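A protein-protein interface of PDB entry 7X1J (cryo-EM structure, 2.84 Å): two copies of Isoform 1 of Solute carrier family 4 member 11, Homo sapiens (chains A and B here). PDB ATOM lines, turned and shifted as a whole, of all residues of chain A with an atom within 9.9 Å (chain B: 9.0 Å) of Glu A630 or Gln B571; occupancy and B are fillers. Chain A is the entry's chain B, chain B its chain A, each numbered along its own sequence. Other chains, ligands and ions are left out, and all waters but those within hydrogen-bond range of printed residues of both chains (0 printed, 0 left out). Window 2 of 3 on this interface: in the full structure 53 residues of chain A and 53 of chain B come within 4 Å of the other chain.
OH of Tyr B518 is in hydrogen-bond range of OE1 of Glu A630 (3.0 Å). OE1 of Gln B571 sits close to O of Glu A630 (3.4 Å).
O of Ile A623 is in hydrogen-bond range of N of Phe A628 (3.0 Å).
Gln A571 touches Ile B631. Ala A572 touches Ala B572 (CB to N, 3.6 Å). CG1 of Val A575 touches CG1 of Val B575 (3.7 Å). CA of Leu B576 touches CG1 of Val A575 (3.6 Å). CG2 of Val A575 touches CD1 of Ile B631 (3.3 Å). Leu A579 touches Leu B578 (CD2 to CD2, 3.8 Å). Phe A628 touches Tyr B518. Val B575 touches Phe A628. Ile A631 touches Tyr B518. CG2 of Val B575 touches CD1 of Ile A631 (3.3 Å).
Of the printed residues of chain B, Gln A571 touches Ile B631 (3.2 Å). Thr A573 touches none of the printed residues of chain B. Printed residues of chain B within 4 Å of Phe A628: Tyr B518 and Val B575. Of the printed residues of chain B, Glu A630 touches Tyr B518 and Gln B571. Gln B571 touches just these residues of chain A: Glu A630 (3.2 Å) and Ile A631 (3.2 Å). Of the printed residues of chain A, Ala B572 touches Ala A572 (3.6 Å). No residue of chain A comes within 4 Å of Ala B574. The nearest residue of chain A that does not touch Gln B571 is Ala A572 (4.03 Å).
Hydrophobic or aromatic side chains of chain A that line the printed part of chain B: Ala A572, Val A575, Leu A576, Leu A579, Phe A628 and Ile A631. Of the 19 printed residues of chain B, 7 touch a printed residue of chain A. Hydrophobic or aromatic side chains of chain B that line the printed part of chain A: Tyr B518, Ala B572, Val B575, Leu B576, Leu B578 and Ile B631. Among the printed residues, 14 pairs touch across the chains. Among the printed residues, no Asp or Glu carboxylate lies within 4 Å of a Lys or Arg side-chain nitrogen of the other chain.
Gln A571 touches Ile B631, and with the chains exchanged Ile A631 touches Gln B571. Ala B572 touches its own counterpart, Ala A572. Val A575 touches its own counterpart, Val B575. Val A575 touches Leu B576, and with the chains exchanged Leu A576 touches Val B575. Of the 14 pairs that touch across the chains among the printed residues, 8 have their exchanged pair printed and touching as well.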
ATOM      1  N   GLY A 570     -18.761   8.594 -20.672  1.00  0.00           N
ATOM      2  CA  GLY A 570     -19.239   8.388 -22.027  1.00  0.00           C
ATOM      3  C   GLY A 570     -20.618   7.760 -22.102  1.00  0.00           C
ATOM      4  O   GLY A 570     -21.630   8.463 -22.061  1.00  0.00           O
ATOM      5  N   GLN A 571     -20.656   6.430 -22.220  1.00  0.00           N
ATOM      6  CA  GLN A 571     -21.933   5.728 -22.318  1.00  0.00           C
ATOM      7  C   GLN A 571     -22.739   5.863 -21.033  1.00  0.00           C
ATOM      8  O   GLN A 571     -23.970   5.971 -21.075  1.00  0.00           O
ATOM      9  CB  GLN A 571     -21.701   4.254 -22.656  1.00  0.00           C
ATOM     10  CG  GLN A 571     -21.096   4.011 -24.033  1.00  0.00           C
ATOM     11  CD  GLN A 571     -20.912   2.536 -24.340  1.00  0.00           C
ATOM     12  OE1 GLN A 571     -21.020   1.686 -23.456  1.00  0.00           O
ATOM     13  NE2 GLN A 571     -20.635   2.225 -25.601  1.00  0.00           N
ATOM     14  N   ALA A 572     -22.064   5.857 -19.882  1.00  0.00           N
ATOM     15  CA  ALA A 572     -22.764   6.012 -18.610  1.00  0.00           C
ATOM     16  C   ALA A 572     -23.463   7.364 -18.524  1.00  0.00           C
ATOM     17  O   ALA A 572     -24.575   7.462 -17.992  1.00  0.00           O
ATOM     18  CB  ALA A 572     -21.788   5.839 -17.447  1.00  0.00           C
ATOM     19  N   THR A 573     -22.822   8.417 -19.035  1.00  0.00           N
ATOM     20  CA  THR A 573     -23.430   9.744 -19.010  1.00  0.00           C
ATOM     21  C   THR A 573     -24.741   9.769 -19.790  1.00  0.00           C
ATOM     22  O   THR A 573     -25.757  10.280 -19.304  1.00  0.00           O
ATOM     23  CB  THR A 573     -22.453  10.777 -19.576  1.00  0.00           C
ATOM     24  OG1 THR A 573     -21.325  10.904 -18.697  1.00  0.00           O
ATOM     25  CG2 THR A 573     -23.131  12.133 -19.729  1.00  0.00           C
ATOM     26  N   ALA A 574     -24.740   9.214 -21.005  1.00  0.00           N
ATOM     27  CA  ALA A 574     -25.951   9.214 -21.821  1.00  0.00           C
ATOM     28  C   ALA A 574     -27.054   8.374 -21.191  1.00  0.00           C
ATOM     29  O   ALA A 574     -28.221   8.782 -21.169  1.00  0.00           O
ATOM     30  CB  ALA A 574     -25.634   8.715 -23.230  1.00  0.00           C
ATOM     31  N   VAL A 575     -26.707   7.188 -20.687  1.00  0.00           N
ATOM     32  CA  VAL A 575     -27.705   6.324 -20.063  1.00  0.00           C
ATOM     33  C   VAL A 575     -28.277   6.985 -18.815  1.00  0.00           C
ATOM     34  O   VAL A 575     -29.493   6.963 -18.585  1.00  0.00           O
ATOM     35  CB  VAL A 575     -27.098   4.944 -19.751  1.00  0.00           C
ATOM     36  CG1 VAL A 575     -28.078   4.099 -18.954  1.00  0.00           C
ATOM     37  CG2 VAL A 575     -26.708   4.233 -21.040  1.00  0.00           C
ATOM     38  N   LEU A 576     -27.413   7.583 -17.993  1.00  0.00           N
ATOM     39  CA  LEU A 576     -27.889   8.299 -16.814  1.00  0.00           C
ATOM     40  C   LEU A 576     -28.718   9.515 -17.209  1.00  0.00           C
ATOM     41  O   LEU A 576     -29.698   9.854 -16.533  1.00  0.00           O
ATOM     42  CB  LEU A 576     -26.708   8.710 -15.936  1.00  0.00           C
ATOM     43  CG  LEU A 576     -27.053   9.334 -14.582  1.00  0.00           C
ATOM     44  CD1 LEU A 576     -27.969   8.412 -13.794  1.00  0.00           C
ATOM     45  CD2 LEU A 576     -25.788   9.639 -13.800  1.00  0.00           C
ATOM     46  N   LEU A 579     -32.099   8.292 -17.823  1.00  0.00           N
ATOM     47  CA  LEU A 579     -32.721   7.917 -16.557  1.00  0.00           C
ATOM     48  C   LEU A 579     -33.149   9.144 -15.761  1.00  0.00           C
ATOM     49  O   LEU A 579     -34.248   9.173 -15.196  1.00  0.00           O
ATOM     50  CB  LEU A 579     -31.760   7.057 -15.739  1.00  0.00           C
ATOM     51  CG  LEU A 579     -32.231   6.624 -14.350  1.00  0.00           C
ATOM     52  CD1 LEU A 579     -33.491   5.777 -14.450  1.00  0.00           C
ATOM     53  CD2 LEU A 579     -31.129   5.873 -13.616  1.00  0.00           C
ATOM     54  N   LEU A 622     -29.935  16.365  -6.726  1.00  0.00           N
ATOM     55  CA  LEU A 622     -29.100  15.701  -5.732  1.00  0.00           C
ATOM     56  C   LEU A 622     -28.690  14.309  -6.197  1.00  0.00           C
ATOM     57  O   LEU A 622     -27.552  13.881  -5.974  1.00  0.00           O
ATOM     58  CB  LEU A 622     -29.836  15.625  -4.394  1.00  0.00           C
ATOM     59  CG  LEU A 622     -30.178  16.956  -3.719  1.00  0.00           C
ATOM     60  CD1 LEU A 622     -30.990  16.724  -2.454  1.00  0.00           C
ATOM     61  CD2 LEU A 622     -28.910  17.737  -3.411  1.00  0.00           C
ATOM     62  N   ILE A 623     -29.612  13.583  -6.833  1.00  0.00           N
ATOM     63  CA  ILE A 623     -29.310  12.230  -7.296  1.00  0.00           C
ATOM     64  C   ILE A 623     -28.205  12.259  -8.345  1.00  0.00           C
ATOM     65  O   ILE A 623     -27.239  11.489  -8.280  1.00  0.00           O
ATOM     66  CB  ILE A 623     -30.580  11.549  -7.833  1.00  0.00           C
ATOM     67  CG1 ILE A 623     -31.582  11.313  -6.701  1.00  0.00           C
ATOM     68  CG2 ILE A 623     -30.238  10.242  -8.531  1.00  0.00           C
ATOM     69  CD1 ILE A 623     -32.855  10.631  -7.148  1.00  0.00           C
ATOM     70  N   SER A 624     -28.327  13.152  -9.329  1.00  0.00           N
ATOM     71  CA  SER A 624     -27.342  13.197 -10.404  1.00  0.00           C
ATOM     72  C   SER A 624     -26.017  13.784  -9.928  1.00  0.00           C
ATOM     73  O   SER A 624     -24.949  13.238 -10.229  1.00  0.00           O
ATOM     74  CB  SER A 624     -27.892  14.001 -11.582  1.00  0.00           C
ATOM     75  OG  SER A 624     -28.181  15.335 -11.198  1.00  0.00           O
ATOM     76  N   SER A 625     -26.063  14.892  -9.188  1.00  0.00           N
ATOM     77  CA  SER A 625     -24.831  15.573  -8.803  1.00  0.00           C
ATOM     78  C   SER A 625     -24.115  14.869  -7.656  1.00  0.00           C
ATOM     79  O   SER A 625     -22.882  14.784  -7.653  1.00  0.00           O
ATOM     80  CB  SER A 625     -25.129  17.026  -8.430  1.00  0.00           C
ATOM     81  OG  SER A 625     -25.661  17.736  -9.534  1.00  0.00           O
ATOM     82  N   HIS A 626     -24.861  14.360  -6.678  1.00  0.00           N
ATOM     83  CA  HIS A 626     -24.276  13.772  -5.477  1.00  0.00           C
ATOM     84  C   HIS A 626     -24.348  12.255  -5.447  1.00  0.00           C
ATOM     85  O   HIS A 626     -23.378  11.606  -5.049  1.00  0.00           O
ATOM     86  CB  HIS A 626     -24.961  14.334  -4.224  1.00  0.00           C
ATOM     87  CG  HIS A 626     -24.310  13.920  -2.941  1.00  0.00           C
ATOM     88  ND1 HIS A 626     -24.588  12.722  -2.318  1.00  0.00           N
ATOM     89  CD2 HIS A 626     -23.397  14.546  -2.163  1.00  0.00           C
ATOM     90  CE1 HIS A 626     -23.872  12.627  -1.212  1.00  0.00           C
ATOM     91  NE2 HIS A 626     -23.141  13.721  -1.095  1.00  0.00           N
ATOM     92  N   GLY A 627     -25.474  11.666  -5.852  1.00  0.00           N
ATOM     93  CA  GLY A 627     -25.573  10.217  -5.889  1.00  0.00           C
ATOM     94  C   GLY A 627     -24.778   9.574  -7.005  1.00  0.00           C
ATOM     95  O   GLY A 627     -24.475   8.380  -6.926  1.00  0.00           O
ATOM     96  N   PHE A 628     -24.439  10.336  -8.043  1.00  0.00           N
ATOM     97  CA  PHE A 628     -23.686   9.848  -9.193  1.00  0.00           C
ATOM     98  C   PHE A 628     -22.499  10.764  -9.475  1.00  0.00           C
ATOM     99  O   PHE A 628     -22.290  11.230 -10.597  1.00  0.00           O
ATOM    100  CB  PHE A 628     -24.583   9.724 -10.420  1.00  0.00           C
ATOM    101  CG  PHE A 628     -25.593   8.616 -10.321  1.00  0.00           C
ATOM    102  CD1 PHE A 628     -25.226   7.304 -10.574  1.00  0.00           C
ATOM    103  CD2 PHE A 628     -26.909   8.884  -9.982  1.00  0.00           C
ATOM    104  CE1 PHE A 628     -26.153   6.280 -10.488  1.00  0.00           C
ATOM    105  CE2 PHE A 628     -27.840   7.865  -9.895  1.00  0.00           C
ATOM    106  CZ  PHE A 628     -27.461   6.562 -10.148  1.00  0.00           C
ATOM    107  N   ARG A 629     -21.710  11.041  -8.432  1.00  0.00           N
ATOM    108  CA  ARG A 629     -20.534  11.892  -8.590  1.00  0.00           C
ATOM    109  C   ARG A 629     -19.540  11.295  -9.578  1.00  0.00           C
ATOM    110  O   ARG A 629     -18.910  12.023 -10.353  1.00  0.00           O
ATOM    111  CB  ARG A 629     -19.866  12.113  -7.234  1.00  0.00           C
ATOM    112  CG  ARG A 629     -20.700  12.907  -6.246  1.00  0.00           C
ATOM    113  CD  ARG A 629     -20.274  12.629  -4.815  1.00  0.00           C
ATOM    114  NE  ARG A 629     -20.513  11.240  -4.442  1.00  0.00           N
ATOM    115  CZ  ARG A 629     -20.309  10.741  -3.232  1.00  0.00           C
ATOM    116  NH1 ARG A 629     -19.855  11.492  -2.242  1.00  0.00           N
ATOM    117  NH2 ARG A 629     -20.568   9.456  -3.008  1.00  0.00           N
ATOM    118  N   GLU A 630     -19.383   9.969  -9.561  1.00  0.00           N
ATOM    119  CA  GLU A 630     -18.407   9.315 -10.425  1.00  0.00           C
ATOM    120  C   GLU A 630     -18.759   9.424 -11.902  1.00  0.00           C
ATOM    121  O   GLU A 630     -17.884   9.216 -12.749  1.00  0.00           O
ATOM    122  CB  GLU A 630     -18.265   7.839 -10.040  1.00  0.00           C
ATOM    123  CG  GLU A 630     -17.751   7.593  -8.626  1.00  0.00           C
ATOM    124  CD  GLU A 630     -18.831   7.737  -7.569  1.00  0.00           C
ATOM    125  OE1 GLU A 630     -20.009   7.918  -7.938  1.00  0.00           O
ATOM    126  OE2 GLU A 630     -18.500   7.672  -6.365  1.00  0.00           O
ATOM    127  N   ILE A 631     -20.007   9.743 -12.234  1.00  0.00           N
ATOM    128  CA  ILE A 631     -20.452   9.846 -13.618  1.00  0.00           C
ATOM    129  C   ILE A 631     -20.606  11.324 -13.952  1.00  0.00           C
ATOM    130  O   ILE A 631     -21.488  12.004 -13.414  1.00  0.00           O
ATOM    131  CB  ILE A 631     -21.763   9.086 -13.853  1.00  0.00           C
ATOM    132  CG1 ILE A 631     -21.589   7.604 -13.514  1.00  0.00           C
ATOM    133  CG2 ILE A 631     -22.226   9.252 -15.291  1.00  0.00           C
ATOM    134  CD1 ILE A 631     -22.854   6.787 -13.673  1.00  0.00           C
ATOM    135  N   GLU A 632     -19.747  11.823 -14.838  1.00  0.00           N
ATOM    136  CA  GLU A 632     -19.840  13.210 -15.272  1.00  0.00           C
ATOM    137  C   GLU A 632     -21.083  13.414 -16.131  1.00  0.00           C
ATOM    138  O   GLU A 632     -21.441  12.563 -16.951  1.00  0.00           O
ATOM    139  CB  GLU A 632     -18.582  13.612 -16.043  1.00  0.00           C
ATOM    140  CG  GLU A 632     -18.215  12.683 -17.192  1.00  0.00           C
ATOM    141  CD  GLU A 632     -18.797  13.127 -18.521  1.00  0.00           C
ATOM    142  OE1 GLU A 632     -19.382  14.230 -18.578  1.00  0.00           O
ATOM    143  OE2 GLU A 632     -18.667  12.374 -19.507  1.00  0.00           O
ATOM    144  N   MET A 633     -21.741  14.553 -15.937  1.00  0.00           N
ATOM    145  CA  MET A 633     -22.994  14.867 -16.609  1.00  0.00           C
ATOM    146  C   MET A 633     -22.851  16.163 -17.394  1.00  0.00           C
ATOM    147  O   MET A 633     -22.144  17.082 -16.969  1.00  0.00           O
ATOM    148  CB  MET A 633     -24.140  14.996 -15.600  1.00  0.00           C
ATOM    149  CG  MET A 633     -24.466  13.708 -14.867  1.00  0.00           C
ATOM    150  SD  MET A 633     -25.330  12.526 -15.917  1.00  0.00           S
ATOM    151  CE  MET A 633     -26.909  13.346 -16.104  1.00  0.00           C
ATOM    152  N   ILE B 513     -25.358  -5.658  -8.591  1.00  0.00           N
ATOM    153  CA  ILE B 513     -24.868  -5.169  -9.880  1.00  0.00           C
ATOM    154  C   ILE B 513     -24.055  -3.894  -9.688  1.00  0.00           C
ATOM    155  O   ILE B 513     -22.973  -3.731 -10.264  1.00  0.00           O
ATOM    156  CB  ILE B 513     -26.039  -4.947 -10.853  1.00  0.00           C
ATOM    157  CG1 ILE B 513     -26.765  -6.266 -11.130  1.00  0.00           C
ATOM    158  CG2 ILE B 513     -25.542  -4.333 -12.156  1.00  0.00           C
ATOM    159  CD1 ILE B 513     -27.938  -6.127 -12.078  1.00  0.00           C
ATOM    160  N   PHE B 514     -24.569  -2.968  -8.875  1.00  0.00           N
ATOM    161  CA  PHE B 514     -23.845  -1.727  -8.610  1.00  0.00           C
ATOM    162  C   PHE B 514     -22.509  -2.000  -7.928  1.00  0.00           C
ATOM    163  O   PHE B 514     -21.490  -1.398  -8.282  1.00  0.00           O
ATOM    164  CB  PHE B 514     -24.700  -0.791  -7.756  1.00  0.00           C
ATOM    165  CG  PHE B 514     -25.546   0.155  -8.558  1.00  0.00           C
ATOM    166  CD1 PHE B 514     -26.781  -0.239  -9.051  1.00  0.00           C
ATOM    167  CD2 PHE B 514     -25.107   1.442  -8.820  1.00  0.00           C
ATOM    168  CE1 PHE B 514     -27.558   0.635  -9.791  1.00  0.00           C
ATOM    169  CE2 PHE B 514     -25.880   2.318  -9.560  1.00  0.00           C
ATOM    170  CZ  PHE B 514     -27.106   1.913 -10.045  1.00  0.00           C
ATOM    171  N   LYS B 516     -20.670  -4.751  -8.084  1.00  0.00           N
ATOM    172  CA  LYS B 516     -19.738  -5.422  -8.985  1.00  0.00           C
ATOM    173  C   LYS B 516     -19.284  -4.506 -10.115  1.00  0.00           C
ATOM    174  O   LYS B 516     -18.097  -4.480 -10.461  1.00  0.00           O
ATOM    175  CB  LYS B 516     -20.375  -6.691  -9.549  1.00  0.00           C
ATOM    176  CG  LYS B 516     -19.471  -7.480 -10.487  1.00  0.00           C
ATOM    177  CD  LYS B 516     -20.175  -8.715 -11.030  1.00  0.00           C
ATOM    178  CE  LYS B 516     -19.265  -9.509 -11.953  1.00  0.00           C
ATOM    179  NZ  LYS B 516     -18.805  -8.698 -13.112  1.00  0.00           N
ATOM    180  N   TYR B 517     -20.208  -3.743 -10.704  1.00  0.00           N
ATOM    181  CA  TYR B 517     -19.926  -2.978 -11.915  1.00  0.00           C
ATOM    182  C   TYR B 517     -19.634  -1.508 -11.631  1.00  0.00           C
ATOM    183  O   TYR B 517     -18.588  -0.993 -12.037  1.00  0.00           O
ATOM    184  CB  TYR B 517     -21.097  -3.105 -12.900  1.00  0.00           C
ATOM    185  CG  TYR B 517     -21.221  -4.474 -13.532  1.00  0.00           C
ATOM    186  CD1 TYR B 517     -20.492  -4.803 -14.668  1.00  0.00           C
ATOM    187  CD2 TYR B 517     -22.063  -5.436 -12.993  1.00  0.00           C
ATOM    188  CE1 TYR B 517     -20.600  -6.052 -15.249  1.00  0.00           C
ATOM    189  CE2 TYR B 517     -22.178  -6.688 -13.567  1.00  0.00           C
ATOM    190  CZ  TYR B 517     -21.445  -6.992 -14.694  1.00  0.00           C
ATOM    191  OH  TYR B 517     -21.557  -8.237 -15.267  1.00  0.00           O
ATOM    192  N   TYR B 518     -20.554  -0.814 -10.953  1.00  0.00           N
ATOM    193  CA  TYR B 518     -20.387   0.621 -10.742  1.00  0.00           C
ATOM    194  C   TYR B 518     -19.147   0.922  -9.908  1.00  0.00           C
ATOM    195  O   TYR B 518     -18.386   1.844 -10.225  1.00  0.00           O
ATOM    196  CB  TYR B 518     -21.636   1.201 -10.077  1.00  0.00           C
ATOM    197  CG  TYR B 518     -21.690   2.712 -10.072  1.00  0.00           C
ATOM    198  CD1 TYR B 518     -22.239   3.410 -11.141  1.00  0.00           C
ATOM    199  CD2 TYR B 518     -21.201   3.441  -8.996  1.00  0.00           C
ATOM    200  CE1 TYR B 518     -22.293   4.792 -11.140  1.00  0.00           C
ATOM    201  CE2 TYR B 518     -21.250   4.821  -8.987  1.00  0.00           C
ATOM    202  CZ  TYR B 518     -21.797   5.492 -10.061  1.00  0.00           C
ATOM    203  OH  TYR B 518     -21.850   6.866 -10.058  1.00  0.00           O
ATOM    204  N   TYR B 519     -18.924   0.155  -8.845  1.00  0.00           N
ATOM    205  CA  TYR B 519     -17.770   0.351  -7.979  1.00  0.00           C
ATOM    206  C   TYR B 519     -16.586  -0.532  -8.351  1.00  0.00           C
ATOM    207  O   TYR B 519     -15.551  -0.468  -7.680  1.00  0.00           O
ATOM    208  CB  TYR B 519     -18.162   0.112  -6.518  1.00  0.00           C
ATOM    209  CG  TYR B 519     -19.245   1.042  -6.023  1.00  0.00           C
ATOM    210  CD1 TYR B 519     -18.943   2.333  -5.610  1.00  0.00           C
ATOM    211  CD2 TYR B 519     -20.570   0.630  -5.969  1.00  0.00           C
ATOM    212  CE1 TYR B 519     -19.928   3.187  -5.157  1.00  0.00           C
ATOM    213  CE2 TYR B 519     -21.563   1.478  -5.519  1.00  0.00           C
ATOM    214  CZ  TYR B 519     -21.237   2.756  -5.115  1.00  0.00           C
ATOM    215  OH  TYR B 519     -22.223   3.604  -4.664  1.00  0.00           O
ATOM    216  N   GLY B 520     -16.711  -1.343  -9.399  1.00  0.00           N
ATOM    217  CA  GLY B 520     -15.594  -2.147  -9.866  1.00  0.00           C
ATOM    218  C   GLY B 520     -15.137  -3.221  -8.905  1.00  0.00           C
ATOM    219  O   GLY B 520     -13.933  -3.484  -8.809  1.00  0.00           O
ATOM    220  N   GLY B 570     -18.910  -0.972 -17.134  1.00  0.00           N
ATOM    221  CA  GLY B 570     -18.814  -0.733 -15.705  1.00  0.00           C
ATOM    222  C   GLY B 570     -19.945   0.111 -15.147  1.00  0.00           C
ATOM    223  O   GLY B 570     -21.002  -0.414 -14.790  1.00  0.00           O
ATOM    224  N   GLN B 571     -19.716   1.425 -15.066  1.00  0.00           N
ATOM    225  CA  GLN B 571     -20.732   2.325 -14.527  1.00  0.00           C
ATOM    226  C   GLN B 571     -21.966   2.364 -15.420  1.00  0.00           C
ATOM    227  O   GLN B 571     -23.094   2.460 -14.923  1.00  0.00           O
ATOM    228  CB  GLN B 571     -20.151   3.728 -14.345  1.00  0.00           C
ATOM    229  CG  GLN B 571     -19.051   3.824 -13.296  1.00  0.00           C
ATOM    230  CD  GLN B 571     -18.526   5.238 -13.125  1.00  0.00           C
ATOM    231  OE1 GLN B 571     -18.810   6.122 -13.934  1.00  0.00           O
ATOM    232  NE2 GLN B 571     -17.757   5.459 -12.066  1.00  0.00           N
ATOM    233  N   ALA B 572     -21.771   2.296 -16.738  1.00  0.00           N
ATOM    234  CA  ALA B 572     -22.905   2.299 -17.656  1.00  0.00           C
ATOM    235  C   ALA B 572     -23.801   1.085 -17.435  1.00  0.00           C
ATOM    236  O   ALA B 572     -25.030   1.189 -17.517  1.00  0.00           O
ATOM    237  CB  ALA B 572     -22.414   2.346 -19.102  1.00  0.00           C
ATOM    238  N   THR B 573     -23.200  -0.075 -17.163  1.00  0.00           N
ATOM    239  CA  THR B 573     -23.984  -1.283 -16.920  1.00  0.00           C
ATOM    240  C   THR B 573     -24.901  -1.115 -15.712  1.00  0.00           C
ATOM    241  O   THR B 573     -26.093  -1.436 -15.774  1.00  0.00           O
ATOM    242  CB  THR B 573     -23.053  -2.480 -16.723  1.00  0.00           C
ATOM    243  OG1 THR B 573     -22.366  -2.764 -17.951  1.00  0.00           O
ATOM    244  CG2 THR B 573     -23.840  -3.710 -16.287  1.00  0.00           C
ATOM    245  N   ALA B 574     -24.360  -0.607 -14.601  1.00  0.00           N
ATOM    246  CA  ALA B 574     -25.167  -0.434 -13.397  1.00  0.00           C
ATOM    247  C   ALA B 574     -26.269   0.597 -13.603  1.00  0.00           C
ATOM    248  O   ALA B 574     -27.413   0.388 -13.179  1.00  0.00           O
ATOM    249  CB  ALA B 574     -24.276  -0.038 -12.220  1.00  0.00           C
ATOM    250  N   VAL B 575     -25.942   1.725 -14.236  1.00  0.00           N
ATOM    251  CA  VAL B 575     -26.942   2.761 -14.475  1.00  0.00           C
ATOM    252  C   VAL B 575     -28.034   2.244 -15.403  1.00  0.00           C
ATOM    253  O   VAL B 575     -29.227   2.474 -15.169  1.00  0.00           O
ATOM    254  CB  VAL B 575     -26.274   4.031 -15.032  1.00  0.00           C
ATOM    255  CG1 VAL B 575     -27.325   5.052 -15.439  1.00  0.00           C
ATOM    256  CG2 VAL B 575     -25.325   4.626 -14.002  1.00  0.00           C
ATOM    257  N   LEU B 576     -27.646   1.537 -16.466  1.00  0.00           N
ATOM    258  CA  LEU B 576     -28.634   0.949 -17.364  1.00  0.00           C
ATOM    259  C   LEU B 576     -29.448  -0.126 -16.653  1.00  0.00           C
ATOM    260  O   LEU B 576     -30.649  -0.276 -16.909  1.00  0.00           O
ATOM    261  CB  LEU B 576     -27.945   0.377 -18.602  1.00  0.00           C
ATOM    262  CG  LEU B 576     -28.862  -0.139 -19.712  1.00  0.00           C
ATOM    263  CD1 LEU B 576     -29.838   0.947 -20.137  1.00  0.00           C
ATOM    264  CD2 LEU B 576     -28.044  -0.623 -20.896  1.00  0.00           C
ATOM    265  N   SER B 577     -28.809  -0.887 -15.759  1.00  0.00           N
ATOM    266  CA  SER B 577     -29.529  -1.900 -14.995  1.00  0.00           C
ATOM    267  C   SER B 577     -30.653  -1.280 -14.171  1.00  0.00           C
ATOM    268  O   SER B 577     -31.761  -1.824 -14.111  1.00  0.00           O
ATOM    269  CB  SER B 577     -28.559  -2.662 -14.091  1.00  0.00           C
ATOM    270  OG  SER B 577     -27.517  -3.254 -14.849  1.00  0.00           O
ATOM    271  N   LEU B 578     -30.381  -0.145 -13.522  1.00  0.00           N
ATOM    272  CA  LEU B 578     -31.431   0.552 -12.784  1.00  0.00           C
ATOM    273  C   LEU B 578     -32.512   1.072 -13.723  1.00  0.00           C
ATOM    274  O   LEU B 578     -33.706   0.990 -13.410  1.00  0.00           O
ATOM    275  CB  LEU B 578     -30.828   1.699 -11.973  1.00  0.00           C
ATOM    276  CG  LEU B 578     -31.791   2.491 -11.087  1.00  0.00           C
ATOM    277  CD1 LEU B 578     -32.392   1.601 -10.011  1.00  0.00           C
ATOM    278  CD2 LEU B 578     -31.083   3.686 -10.466  1.00  0.00           C
ATOM    279  N   ILE B 631     -23.349  -1.630 -24.478  1.00  0.00           N
ATOM    280  CA  ILE B 631     -23.264  -1.703 -23.025  1.00  0.00           C
ATOM    281  C   ILE B 631     -23.525  -3.146 -22.610  1.00  0.00           C
ATOM    282  O   ILE B 631     -24.643  -3.652 -22.764  1.00  0.00           O
ATOM    283  CB  ILE B 631     -24.251  -0.745 -22.347  1.00  0.00           C
ATOM    284  CG1 ILE B 631     -23.972   0.698 -22.773  1.00  0.00           C
ATOM    285  CG2 ILE B 631     -24.172  -0.878 -20.835  1.00  0.00           C
ATOM    286  CD1 ILE B 631     -24.935   1.707 -22.185  1.00  0.00           C
ATOM    287  N   GLU B 632     -22.496  -3.807 -22.088  1.00  0.00           N
ATOM    288  CA  GLU B 632     -22.649  -5.173 -21.607  1.00  0.00           C
ATOM    289  C   GLU B 632     -23.504  -5.197 -20.344  1.00  0.00           C
ATOM    290  O   GLU B 632     -23.389  -4.325 -19.477  1.00  0.00           O
ATOM    291  CB  GLU B 632     -21.281  -5.801 -21.341  1.00  0.00           C
ATOM    292  CG  GLU B 632     -20.368  -4.983 -20.439  1.00  0.00           C
ATOM    293  CD  GLU B 632     -20.484  -5.367 -18.976  1.00  0.00           C
ATOM    294  OE1 GLU B 632     -21.180  -6.359 -18.671  1.00  0.00           O
ATOM    295  OE2 GLU B 632     -19.878  -4.678 -18.131  1.00  0.00           O
ATOM    296  N   MET B 633     -24.366  -6.204 -20.245  1.00  0.00           N
ATOM    297  CA  MET B 633     -25.317  -6.329 -19.150  1.00  0.00           C
ATOM    298  C   MET B 633     -25.110  -7.654 -18.432  1.00  0.00           C
ATOM    299  O   MET B 633     -24.772  -8.664 -19.059  1.00  0.00           O
ATOM    300  CB  MET B 633     -26.758  -6.233 -19.661  1.00  0.00           C
ATOM    301  CG  MET B 633     -27.113  -4.886 -20.263  1.00  0.00           C
ATOM    302  SD  MET B 633     -27.322  -3.612 -19.006  1.00  0.00           S
ATOM    303  CE  MET B 633     -28.833  -4.166 -18.225  1.00  0.00           C
